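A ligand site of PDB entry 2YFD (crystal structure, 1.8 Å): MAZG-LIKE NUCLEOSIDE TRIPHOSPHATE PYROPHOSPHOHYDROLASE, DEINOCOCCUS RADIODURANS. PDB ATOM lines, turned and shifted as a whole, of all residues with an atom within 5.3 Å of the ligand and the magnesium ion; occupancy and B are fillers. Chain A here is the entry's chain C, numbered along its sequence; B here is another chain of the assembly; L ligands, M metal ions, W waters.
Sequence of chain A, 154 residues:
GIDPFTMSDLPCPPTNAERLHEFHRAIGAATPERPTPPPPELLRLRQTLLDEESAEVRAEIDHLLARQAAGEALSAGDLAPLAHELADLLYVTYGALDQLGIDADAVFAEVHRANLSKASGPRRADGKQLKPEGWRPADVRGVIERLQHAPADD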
ATOM      1  N   VAL A 111       4.564  22.843 -17.323  1.00  0.00           N
ATOM      2  CA  VAL A 111       3.096  22.947 -17.348  1.00  0.00           C
ATOM      3  C   VAL A 111       2.614  24.253 -16.707  1.00  0.00           C
ATOM      4  O   VAL A 111       1.728  24.941 -17.224  1.00  0.00           O
ATOM      5  CB  VAL A 111       2.443  21.741 -16.667  1.00  0.00           C
ATOM      6  CG1 VAL A 111       0.936  22.003 -16.413  1.00  0.00           C
ATOM      7  CG2 VAL A 111       2.666  20.457 -17.493  1.00  0.00           C
ATOM      8  N   ASN A 115       0.546  27.466 -18.199  1.00  0.00           N
ATOM      9  CA  ASN A 115      -0.729  27.804 -17.597  1.00  0.00           C
ATOM     10  C   ASN A 115      -0.851  29.299 -17.258  1.00  0.00           C
ATOM     11  O   ASN A 115      -1.845  29.898 -17.365  1.00  0.00           O
ATOM     12  CB  ASN A 115      -1.007  26.927 -16.399  1.00  0.00           C
ATOM     13  CG  ASN A 115      -1.559  25.559 -16.805  1.00  0.00           C
ATOM     14  OD1 ASN A 115      -1.990  25.429 -17.862  1.00  0.00           O
ATOM     15  ND2 ASN A 115      -1.543  24.602 -15.935  1.00  0.00           N
ATOM     16  N   LYS A 118      -2.113  31.557 -19.908  1.00  0.00           N
ATOM     17  CA  LYS A 118      -3.551  31.517 -20.238  1.00  0.00           C
ATOM     18  C   LYS A 118      -4.333  32.699 -19.671  1.00  0.00           C
ATOM     19  O   LYS A 118      -5.524  32.858 -19.978  1.00  0.00           O
ATOM     20  CB  LYS A 118      -4.195  30.238 -19.712  1.00  0.00           C
ATOM     21  CG  LYS A 118      -3.624  28.961 -20.301  1.00  0.00           C
ATOM     22  CD  LYS A 118      -4.302  27.749 -19.669  1.00  0.00           C
ATOM     23  CE  LYS A 118      -3.731  26.471 -20.257  1.00  0.00           C
ATOM     24  NZ  LYS A 118      -4.301  25.267 -19.605  1.00  0.00           N
ATOM     25  N   GLY A 127     -16.301  28.390 -14.666  1.00  0.00           N
ATOM     26  CA  GLY A 127     -15.169  29.057 -14.070  1.00  0.00           C
ATOM     27  C   GLY A 127     -13.842  28.585 -14.653  1.00  0.00           C
ATOM     28  O   GLY A 127     -12.806  29.154 -14.340  1.00  0.00           O
ATOM     29  N   LYS A 128     -13.871  27.548 -15.479  1.00  0.00           N
ATOM     30  CA  LYS A 128     -12.601  27.035 -16.015  1.00  0.00           C
ATOM     31  C   LYS A 128     -11.895  28.094 -16.866  1.00  0.00           C
ATOM     32  O   LYS A 128     -12.514  28.766 -17.708  1.00  0.00           O
ATOM     33  CB  LYS A 128     -12.802  25.756 -16.838  1.00  0.00           C
ATOM     34  CG  LYS A 128     -11.455  25.196 -17.304  1.00  0.00           C
ATOM     35  CD  LYS A 128     -11.650  24.016 -18.258  1.00  0.00           C
ATOM     36  CE  LYS A 128     -10.281  23.403 -18.595  1.00  0.00           C
ATOM     37  NZ  LYS A 128     -10.439  22.208 -19.479  1.00  0.00           N
ATOM     38  N   GLN A 129     -10.597  28.273 -16.634  1.00  0.00           N
ATOM     39  CA  GLN A 129      -9.806  29.186 -17.443  1.00  0.00           C
ATOM     40  C   GLN A 129      -9.536  28.550 -18.816  1.00  0.00           C
ATOM     41  O   GLN A 129      -9.024  27.434 -18.902  1.00  0.00           O
ATOM     42  CB  GLN A 129      -8.455  29.469 -16.763  1.00  0.00           C
ATOM     43  CG  GLN A 129      -7.540  30.438 -17.546  1.00  0.00           C
ATOM     44  CD  GLN A 129      -8.173  31.788 -17.784  1.00  0.00           C
ATOM     45  OE1 GLN A 129      -8.487  32.501 -16.702  1.00  0.00           O
ATOM     46  NE2 GLN A 129      -8.391  32.198 -18.937  1.00  0.00           N
ATOM     47  N   LYS A 131      -8.079  28.976 -23.058  1.00  0.00           N
ATOM     48  CA  LYS A 131      -6.849  29.434 -23.713  1.00  0.00           C
ATOM     49  C   LYS A 131      -7.071  30.627 -24.641  1.00  0.00           C
ATOM     50  O   LYS A 131      -7.991  30.624 -25.463  1.00  0.00           O
ATOM     51  CB  LYS A 131      -6.173  28.270 -24.465  1.00  0.00           C
ATOM     52  CG  LYS A 131      -5.733  27.150 -23.553  1.00  0.00           C
ATOM     53  CD  LYS A 131      -5.834  25.776 -24.202  1.00  0.00           C
ATOM     54  CE  LYS A 131      -5.370  24.683 -23.233  1.00  0.00           C
ATOM     55  NZ  LYS A 131      -5.587  23.324 -23.827  1.00  0.00           N
ATOM     56  N   LEU B  20       0.380  27.044  -7.738  1.00  0.00           N
ATOM     57  CA  LEU B  20      -1.069  27.170  -7.928  1.00  0.00           C
ATOM     58  C   LEU B  20      -1.571  28.518  -7.397  1.00  0.00           C
ATOM     59  O   LEU B  20      -2.471  29.113  -7.987  1.00  0.00           O
ATOM     60  CB  LEU B  20      -1.842  26.038  -7.257  1.00  0.00           C
ATOM     61  CG  LEU B  20      -2.360  24.977  -8.223  1.00  0.00           C
ATOM     62  CD1 LEU B  20      -3.288  25.607  -9.240  1.00  0.00           C
ATOM     63  CD2 LEU B  20      -1.178  24.325  -8.923  1.00  0.00           C
ATOM     64  N   PHE B  23      -0.853  31.055  -9.996  1.00  0.00           N
ATOM     65  CA  PHE B  23      -1.776  30.890 -11.107  1.00  0.00           C
ATOM     66  C   PHE B  23      -3.162  31.478 -10.805  1.00  0.00           C
ATOM     67  O   PHE B  23      -3.712  32.250 -11.595  1.00  0.00           O
ATOM     68  CB  PHE B  23      -1.913  29.400 -11.439  1.00  0.00           C
ATOM     69  CG  PHE B  23      -2.944  29.100 -12.492  1.00  0.00           C
ATOM     70  CD1 PHE B  23      -2.730  29.478 -13.810  1.00  0.00           C
ATOM     71  CD2 PHE B  23      -4.104  28.412 -12.160  1.00  0.00           C
ATOM     72  CE1 PHE B  23      -3.680  29.174 -14.792  1.00  0.00           C
ATOM     73  CE2 PHE B  23      -5.054  28.108 -13.142  1.00  0.00           C
ATOM     74  CZ  PHE B  23      -4.837  28.499 -14.458  1.00  0.00           C
ATOM     75  N   HIS B  24      -3.717  31.129  -9.654  1.00  0.00           N
ATOM     76  CA  HIS B  24      -5.057  31.611  -9.320  1.00  0.00           C
ATOM     77  C   HIS B  24      -5.058  33.135  -9.148  1.00  0.00           C
ATOM     78  O   HIS B  24      -6.005  33.793  -9.561  1.00  0.00           O
ATOM     79  CB  HIS B  24      -5.623  30.874  -8.099  1.00  0.00           C
ATOM     80  CG  HIS B  24      -6.076  29.479  -8.405  1.00  0.00           C
ATOM     81  ND1 HIS B  24      -6.151  28.492  -7.438  1.00  0.00           N
ATOM     82  CD2 HIS B  24      -6.455  28.893  -9.568  1.00  0.00           C
ATOM     83  CE1 HIS B  24      -6.571  27.365  -8.007  1.00  0.00           C
ATOM     84  NE2 HIS B  24      -6.758  27.590  -9.294  1.00  0.00           N
ATOM     85  N   ILE B  27      -5.173  34.635 -12.663  1.00  0.00           N
ATOM     86  CA  ILE B  27      -6.403  34.517 -13.450  1.00  0.00           C
ATOM     87  C   ILE B  27      -7.623  35.052 -12.715  1.00  0.00           C
ATOM     88  O   ILE B  27      -8.741  34.978 -13.225  1.00  0.00           O
ATOM     89  CB  ILE B  27      -6.670  33.076 -13.917  1.00  0.00           C
ATOM     90  CG1 ILE B  27      -7.027  32.159 -12.731  1.00  0.00           C
ATOM     91  CG2 ILE B  27      -5.462  32.511 -14.678  1.00  0.00           C
ATOM     92  CD1 ILE B  27      -7.649  30.823 -13.143  1.00  0.00           C
ATOM     93  N   LEU B  45     -16.817  22.934  -9.870  1.00  0.00           N
ATOM     94  CA  LEU B  45     -15.708  23.156 -10.789  1.00  0.00           C
ATOM     95  C   LEU B  45     -14.542  22.232 -10.473  1.00  0.00           C
ATOM     96  O   LEU B  45     -13.943  21.635 -11.387  1.00  0.00           O
ATOM     97  CB  LEU B  45     -15.224  24.619 -10.776  1.00  0.00           C
ATOM     98  CG  LEU B  45     -13.974  24.837 -11.651  1.00  0.00           C
ATOM     99  CD1 LEU B  45     -14.308  24.640 -13.140  1.00  0.00           C
ATOM    100  CD2 LEU B  45     -13.373  26.226 -11.442  1.00  0.00           C
ATOM    101  N   ARG B  46     -14.181  22.119  -9.196  1.00  0.00           N
ATOM    102  CA  ARG B  46     -13.041  21.259  -8.840  1.00  0.00           C
ATOM    103  C   ARG B  46     -13.292  19.810  -9.283  1.00  0.00           C
ATOM    104  O   ARG B  46     -12.383  19.142  -9.789  1.00  0.00           O
ATOM    105  CB  ARG B  46     -12.700  21.306  -7.346  1.00  0.00           C
ATOM    106  CG  ARG B  46     -12.322  22.697  -6.758  1.00  0.00           C
ATOM    107  CD  ARG B  46     -11.586  23.624  -7.725  1.00  0.00           C
ATOM    108  NE  ARG B  46     -10.352  23.054  -8.307  1.00  0.00           N
ATOM    109  CZ  ARG B  46      -9.518  23.742  -9.073  1.00  0.00           C
ATOM    110  NH1 ARG B  46      -9.751  25.029  -9.330  1.00  0.00           N
ATOM    111  NH2 ARG B  46      -8.444  23.149  -9.585  1.00  0.00           N
ATOM    112  N   LEU B  49     -12.900  19.548 -13.192  1.00  0.00           N
ATOM    113  CA  LEU B  49     -11.498  19.600 -13.603  1.00  0.00           C
ATOM    114  C   LEU B  49     -10.766  18.298 -13.275  1.00  0.00           C
ATOM    115  O   LEU B  49      -9.961  17.809 -14.074  1.00  0.00           O
ATOM    116  CB  LEU B  49     -10.771  20.782 -12.952  1.00  0.00           C
ATOM    117  CG  LEU B  49     -11.290  22.190 -13.305  1.00  0.00           C
ATOM    118  CD1 LEU B  49     -10.432  23.272 -12.637  1.00  0.00           C
ATOM    119  CD2 LEU B  49     -11.351  22.411 -14.823  1.00  0.00           C
ATOM    120  N   GLU B  52     -11.969  15.767 -15.837  1.00  0.00           N
ATOM    121  CA  GLU B  52     -11.366  16.031 -17.135  1.00  0.00           C
ATOM    122  C   GLU B  52      -9.930  15.521 -17.182  1.00  0.00           C
ATOM    123  O   GLU B  52      -9.548  14.801 -18.123  1.00  0.00           O
ATOM    124  CB  GLU B  52     -11.391  17.528 -17.489  1.00  0.00           C
ATOM    125  CG  GLU B  52     -12.797  18.102 -17.711  1.00  0.00           C
ATOM    126  CD  GLU B  52     -12.795  19.585 -18.100  1.00  0.00           C
ATOM    127  OE1 GLU B  52     -11.723  20.219 -18.035  1.00  0.00           O
ATOM    128  OE2 GLU B  52     -13.863  20.104 -18.497  1.00  0.00           O
ATOM    129  N   GLU B  53      -9.118  15.892 -16.199  1.00  0.00           N
ATOM    130  CA  GLU B  53      -7.695  15.535 -16.259  1.00  0.00           C
ATOM    131  C   GLU B  53      -7.491  14.041 -16.006  1.00  0.00           C
ATOM    132  O   GLU B  53      -6.585  13.431 -16.577  1.00  0.00           O
ATOM    133  CB  GLU B  53      -6.833  16.390 -15.313  1.00  0.00           C
ATOM    134  CG  GLU B  53      -6.843  17.899 -15.673  1.00  0.00           C
ATOM    135  CD  GLU B  53      -6.654  18.155 -17.166  1.00  0.00           C
ATOM    136  OE1 GLU B  53      -5.719  17.571 -17.747  1.00  0.00           O
ATOM    137  OE2 GLU B  53      -7.443  18.925 -17.753  1.00  0.00           O
ATOM    138  N   GLU B  56      -8.007  12.233 -19.239  1.00  0.00           N
ATOM    139  CA  GLU B  56      -6.899  12.339 -20.173  1.00  0.00           C
ATOM    140  C   GLU B  56      -5.757  11.417 -19.766  1.00  0.00           C
ATOM    141  O   GLU B  56      -5.110  10.804 -20.618  1.00  0.00           O
ATOM    142  CB  GLU B  56      -6.403  13.772 -20.277  1.00  0.00           C
ATOM    143  CG  GLU B  56      -7.350  14.676 -21.026  1.00  0.00           C
ATOM    144  CD  GLU B  56      -7.114  16.130 -20.696  1.00  0.00           C
ATOM    145  OE1 GLU B  56      -7.331  16.493 -19.527  1.00  0.00           O
ATOM    146  OE2 GLU B  56      -6.696  16.885 -21.593  1.00  0.00           O
ATOM    147  N   GLU B  85      -0.125  14.836 -18.897  1.00  0.00           N
ATOM    148  CA  GLU B  85      -1.455  14.668 -18.287  1.00  0.00           C
ATOM    149  C   GLU B  85      -1.396  14.383 -16.778  1.00  0.00           C
ATOM    150  O   GLU B  85      -2.236  14.845 -16.028  1.00  0.00           O
ATOM    151  CB  GLU B  85      -2.281  13.590 -19.012  1.00  0.00           C
ATOM    152  CG  GLU B  85      -2.496  13.866 -20.524  1.00  0.00           C
ATOM    153  CD  GLU B  85      -3.106  15.235 -20.806  1.00  0.00           C
ATOM    154  OE1 GLU B  85      -3.701  15.825 -19.898  1.00  0.00           O
ATOM    155  OE2 GLU B  85      -3.020  15.738 -21.950  1.00  0.00           O
ATOM    156  N   ALA B  87       0.873  15.574 -14.823  1.00  0.00           N
ATOM    157  CA  ALA B  87       1.163  16.890 -14.241  1.00  0.00           C
ATOM    158  C   ALA B  87      -0.075  17.802 -14.243  1.00  0.00           C
ATOM    159  O   ALA B  87      -0.274  18.572 -13.315  1.00  0.00           O
ATOM    160  CB  ALA B  87       2.320  17.569 -14.958  1.00  0.00           C
ATOM    161  N   ASP B  88      -0.905  17.688 -15.273  1.00  0.00           N
ATOM    162  CA  ASP B  88      -2.173  18.415 -15.308  1.00  0.00           C
ATOM    163  C   ASP B  88      -3.095  17.931 -14.179  1.00  0.00           C
ATOM    164  O   ASP B  88      -3.820  18.739 -13.581  1.00  0.00           O
ATOM    165  CB  ASP B  88      -2.908  18.179 -16.640  1.00  0.00           C
ATOM    166  CG  ASP B  88      -2.425  19.075 -17.752  1.00  0.00           C
ATOM    167  OD1 ASP B  88      -1.644  20.031 -17.537  1.00  0.00           O
ATOM    168  OD2 ASP B  88      -2.855  18.814 -18.892  1.00  0.00           O
ATOM    169  N   TYR B  91      -1.889  19.405 -11.109  1.00  0.00           N
ATOM    170  CA  TYR B  91      -2.200  20.831 -11.168  1.00  0.00           C
ATOM    171  C   TYR B  91      -3.600  21.110 -10.643  1.00  0.00           C
ATOM    172  O   TYR B  91      -3.782  21.999  -9.808  1.00  0.00           O
ATOM    173  CB  TYR B  91      -2.029  21.379 -12.586  1.00  0.00           C
ATOM    174  CG  TYR B  91      -1.652  22.838 -12.617  1.00  0.00           C
ATOM    175  CD1 TYR B  91      -2.625  23.827 -12.564  1.00  0.00           C
ATOM    176  CD2 TYR B  91      -0.319  23.230 -12.667  1.00  0.00           C
ATOM    177  CE1 TYR B  91      -2.268  25.170 -12.585  1.00  0.00           C
ATOM    178  CE2 TYR B  91       0.044  24.550 -12.688  1.00  0.00           C
ATOM    179  CZ  TYR B  91      -0.928  25.519 -12.643  1.00  0.00           C
ATOM    180  OH  TYR B  91      -0.540  26.841 -12.667  1.00  0.00           O
ATOM    181  N   VAL B  92      -4.590  20.342 -11.117  1.00  0.00           N
ATOM    182  CA  VAL B  92      -5.985  20.554 -10.705  1.00  0.00           C
ATOM    183  C   VAL B  92      -6.282  20.026  -9.286  1.00  0.00           C
ATOM    184  O   VAL B  92      -7.220  20.471  -8.629  1.00  0.00           O
ATOM    185  CB  VAL B  92      -7.030  20.013 -11.721  1.00  0.00           C
ATOM    186  CG1 VAL B  92      -6.827  20.624 -13.124  1.00  0.00           C
ATOM    187  CG2 VAL B  92      -7.065  18.466 -11.779  1.00  0.00           C
HETATM  188  N1  LIG L   1      -6.205  24.621 -15.351  1.00  0.00           N
HETATM  189  C1  LIG L   1      -6.496  24.921 -14.081  1.00  0.00           C
HETATM  190  N2  LIG L   1      -7.622  25.690 -13.797  1.00  0.00           N
HETATM  191  C2  LIG L   1      -8.423  26.123 -14.853  1.00  0.00           C
HETATM  192  C3  LIG L   1      -8.128  25.811 -16.179  1.00  0.00           C
HETATM  193  C4  LIG L   1      -7.022  25.057 -16.445  1.00  0.00           C
HETATM  194  O1  LIG L   1      -5.773  24.531 -13.183  1.00  0.00           O
HETATM  195  O2  LIG L   1      -9.521  26.887 -14.538  1.00  0.00           O
HETATM  196  C5  LIG L   1      -5.022  23.842 -15.614  1.00  0.00           C
HETATM  197  C6  LIG L   1      -4.823  22.359 -15.193  1.00  0.00           C
HETATM  198  C7  LIG L   1      -3.938  21.816 -16.247  1.00  0.00           C
HETATM  199  C8  LIG L   1      -4.458  22.542 -17.456  1.00  0.00           C
HETATM  200  O3  LIG L   1      -2.595  21.907 -16.026  1.00  0.00           O
HETATM  201  O4  LIG L   1      -4.598  23.909 -17.051  1.00  0.00           O
HETATM  202  C9  LIG L   1      -5.486  21.874 -18.305  1.00  0.00           C
HETATM  203  O5  LIG L   1      -6.303  22.725 -19.044  1.00  0.00           O
HETATM  204  P1  LIG L   1      -6.961  22.278 -20.399  1.00  0.00           P
HETATM  205  O6  LIG L   1      -7.644  23.437 -21.056  1.00  0.00           O
HETATM  206  O7  LIG L   1      -5.894  21.739 -21.310  1.00  0.00           O
HETATM  207  O8  LIG L   1      -7.983  21.230 -20.084  1.00  0.00           O
HETATM  208 MG    MG M   1      -4.689  17.517 -19.652  1.00  0.00          MG
HETATM  209  O   HOH W   1      -2.623  19.227 -21.485  1.00  0.00           O
HETATM  210  O   HOH W   2      -5.860  19.109 -20.810  1.00  0.00           O
HETATM  211  O   HOH W   3      -6.318  24.752 -10.565  1.00  0.00           O
HETATM  212  O   HOH W   4      -7.073  25.838 -20.054  1.00  0.00           O
HETATM  213  O   HOH W   5      -9.344  24.084 -23.046  1.00  0.00           O
HETATM  214  O   HOH W   6      -3.519  22.994 -20.973  1.00  0.00           O
HETATM  215  O   HOH W   7     -10.344  28.421 -12.437  1.00  0.00           O
HETATM  216  O   HOH W   8      -8.500  26.633 -11.345  1.00  0.00           O
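Val 111 touches the ligand (CG1 to O3, 3.6 Å).
Gly 127 touches the ligand.
Phe 23 of chain B touches the ligand (CE2 to N2, 3.6 Å).
CD1 of Leu 49 of chain B touches N2 of the ligand (3.9 Å).
CD1 of Tyr 91 of chain B touches O1 of the ligand (3.3 Å).
Val 92 of chain B touches the ligand (CG1 to C6, 3.4 Å).
Of the 22 residues printed, 13 come within 4 Å of the ligand.
Water W2 lies within hydrogen-bond range of the side-chain carboxylate of Glu 56 of chain B (2.5 Å), an oxygen (O7) of the ligand (2.7 Å) and the side-chain carboxylate of Glu 53 of chain B (3.4 Å).
Water W4 lies within hydrogen-bond range of O6 of the ligand (2.7 Å), O of Gln 129 (2.8 Å) and NZ of Lys 118 (2.9 Å).
Water W3 lies within hydrogen-bond range of O1 of the ligand (2.7 Å), NH2 of Arg 46 of chain B (2.8 Å) and NE2 of His 24 of chain B (3.1 Å).
Water W6 lies within hydrogen-bond range of O7 of the ligand and NZ of Lys 118.
Water W7 lies within hydrogen-bond range of an oxygen (O2) of the ligand (2.7 Å) and the backbone carbonyl oxygen of Gly 127 (3.2 Å).
Water W8 lies within hydrogen-bond range of a nitrogen (N2) of the ligand, a ring nitrogen (NE2) of His 24 of chain B and the guanidinium group of Arg 46 of chain B.
The magnesium ion is bound by the side-chain carboxylate (OE1) of Glu 85 of chain B (2.0 Å), the side-chain carboxylate (OE1) of Glu 53 of chain B (2.2 Å), water W2 (2.3 Å) and the side-chain carboxylate (OD2) of Asp 88 of chain B (2.4 Å).
Slightly farther from the magnesium ion lies OE1 of Glu 56 of chain B (2.8 Å).
An oxygen (O3) of the ligand lies within hydrogen-bond range of the side-chain carboxylate (OD1) of Asp 88 of chain B, 2.6 Å away.
The side-chain amino group (NZ) of Lys 118 sits at hydrogen-bond distance from an oxygen (O4) of the ligand (2.9 Å).
O8 of the ligand lies within salt-bridge range of NZ of Lys 128, 2.7 Å away.
The side-chain amide nitrogen of Asn 115 lies within hydrogen-bond range of an oxygen (O3) of the ligand, at 2.9 Å.
NZ of Lys 131 is in salt-bridge range of O7 of the ligand (3.0 Å).
N of Gln 129 sits at hydrogen-bond distance from O2 of the ligand, at 2.7 Å.
OD1 of Asn 115 lies within hydrogen-bond range of NZ of Lys 118 (2.9 Å).
The side-chain amide nitrogen (NE2) of Gln 129 lies within hydrogen-bond range of the backbone carbonyl oxygen (O) of Lys 118 (3.1 Å).
The side-chain carboxylate of Glu 56 of chain B lies close to the side-chain carboxylate of Glu 53 of chain B (2.6 Å).
NH2 of Arg 46 of chain B is in hydrogen-bond range of O of Val 92 of chain B (3.1 Å).
NZ of Lys 128 lies within salt-bridge range of OE1 of Glu 52 of chain B (2.8 Å).
Of the 22 residues printed, 4 come within 4 Å of the magnesium ion.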
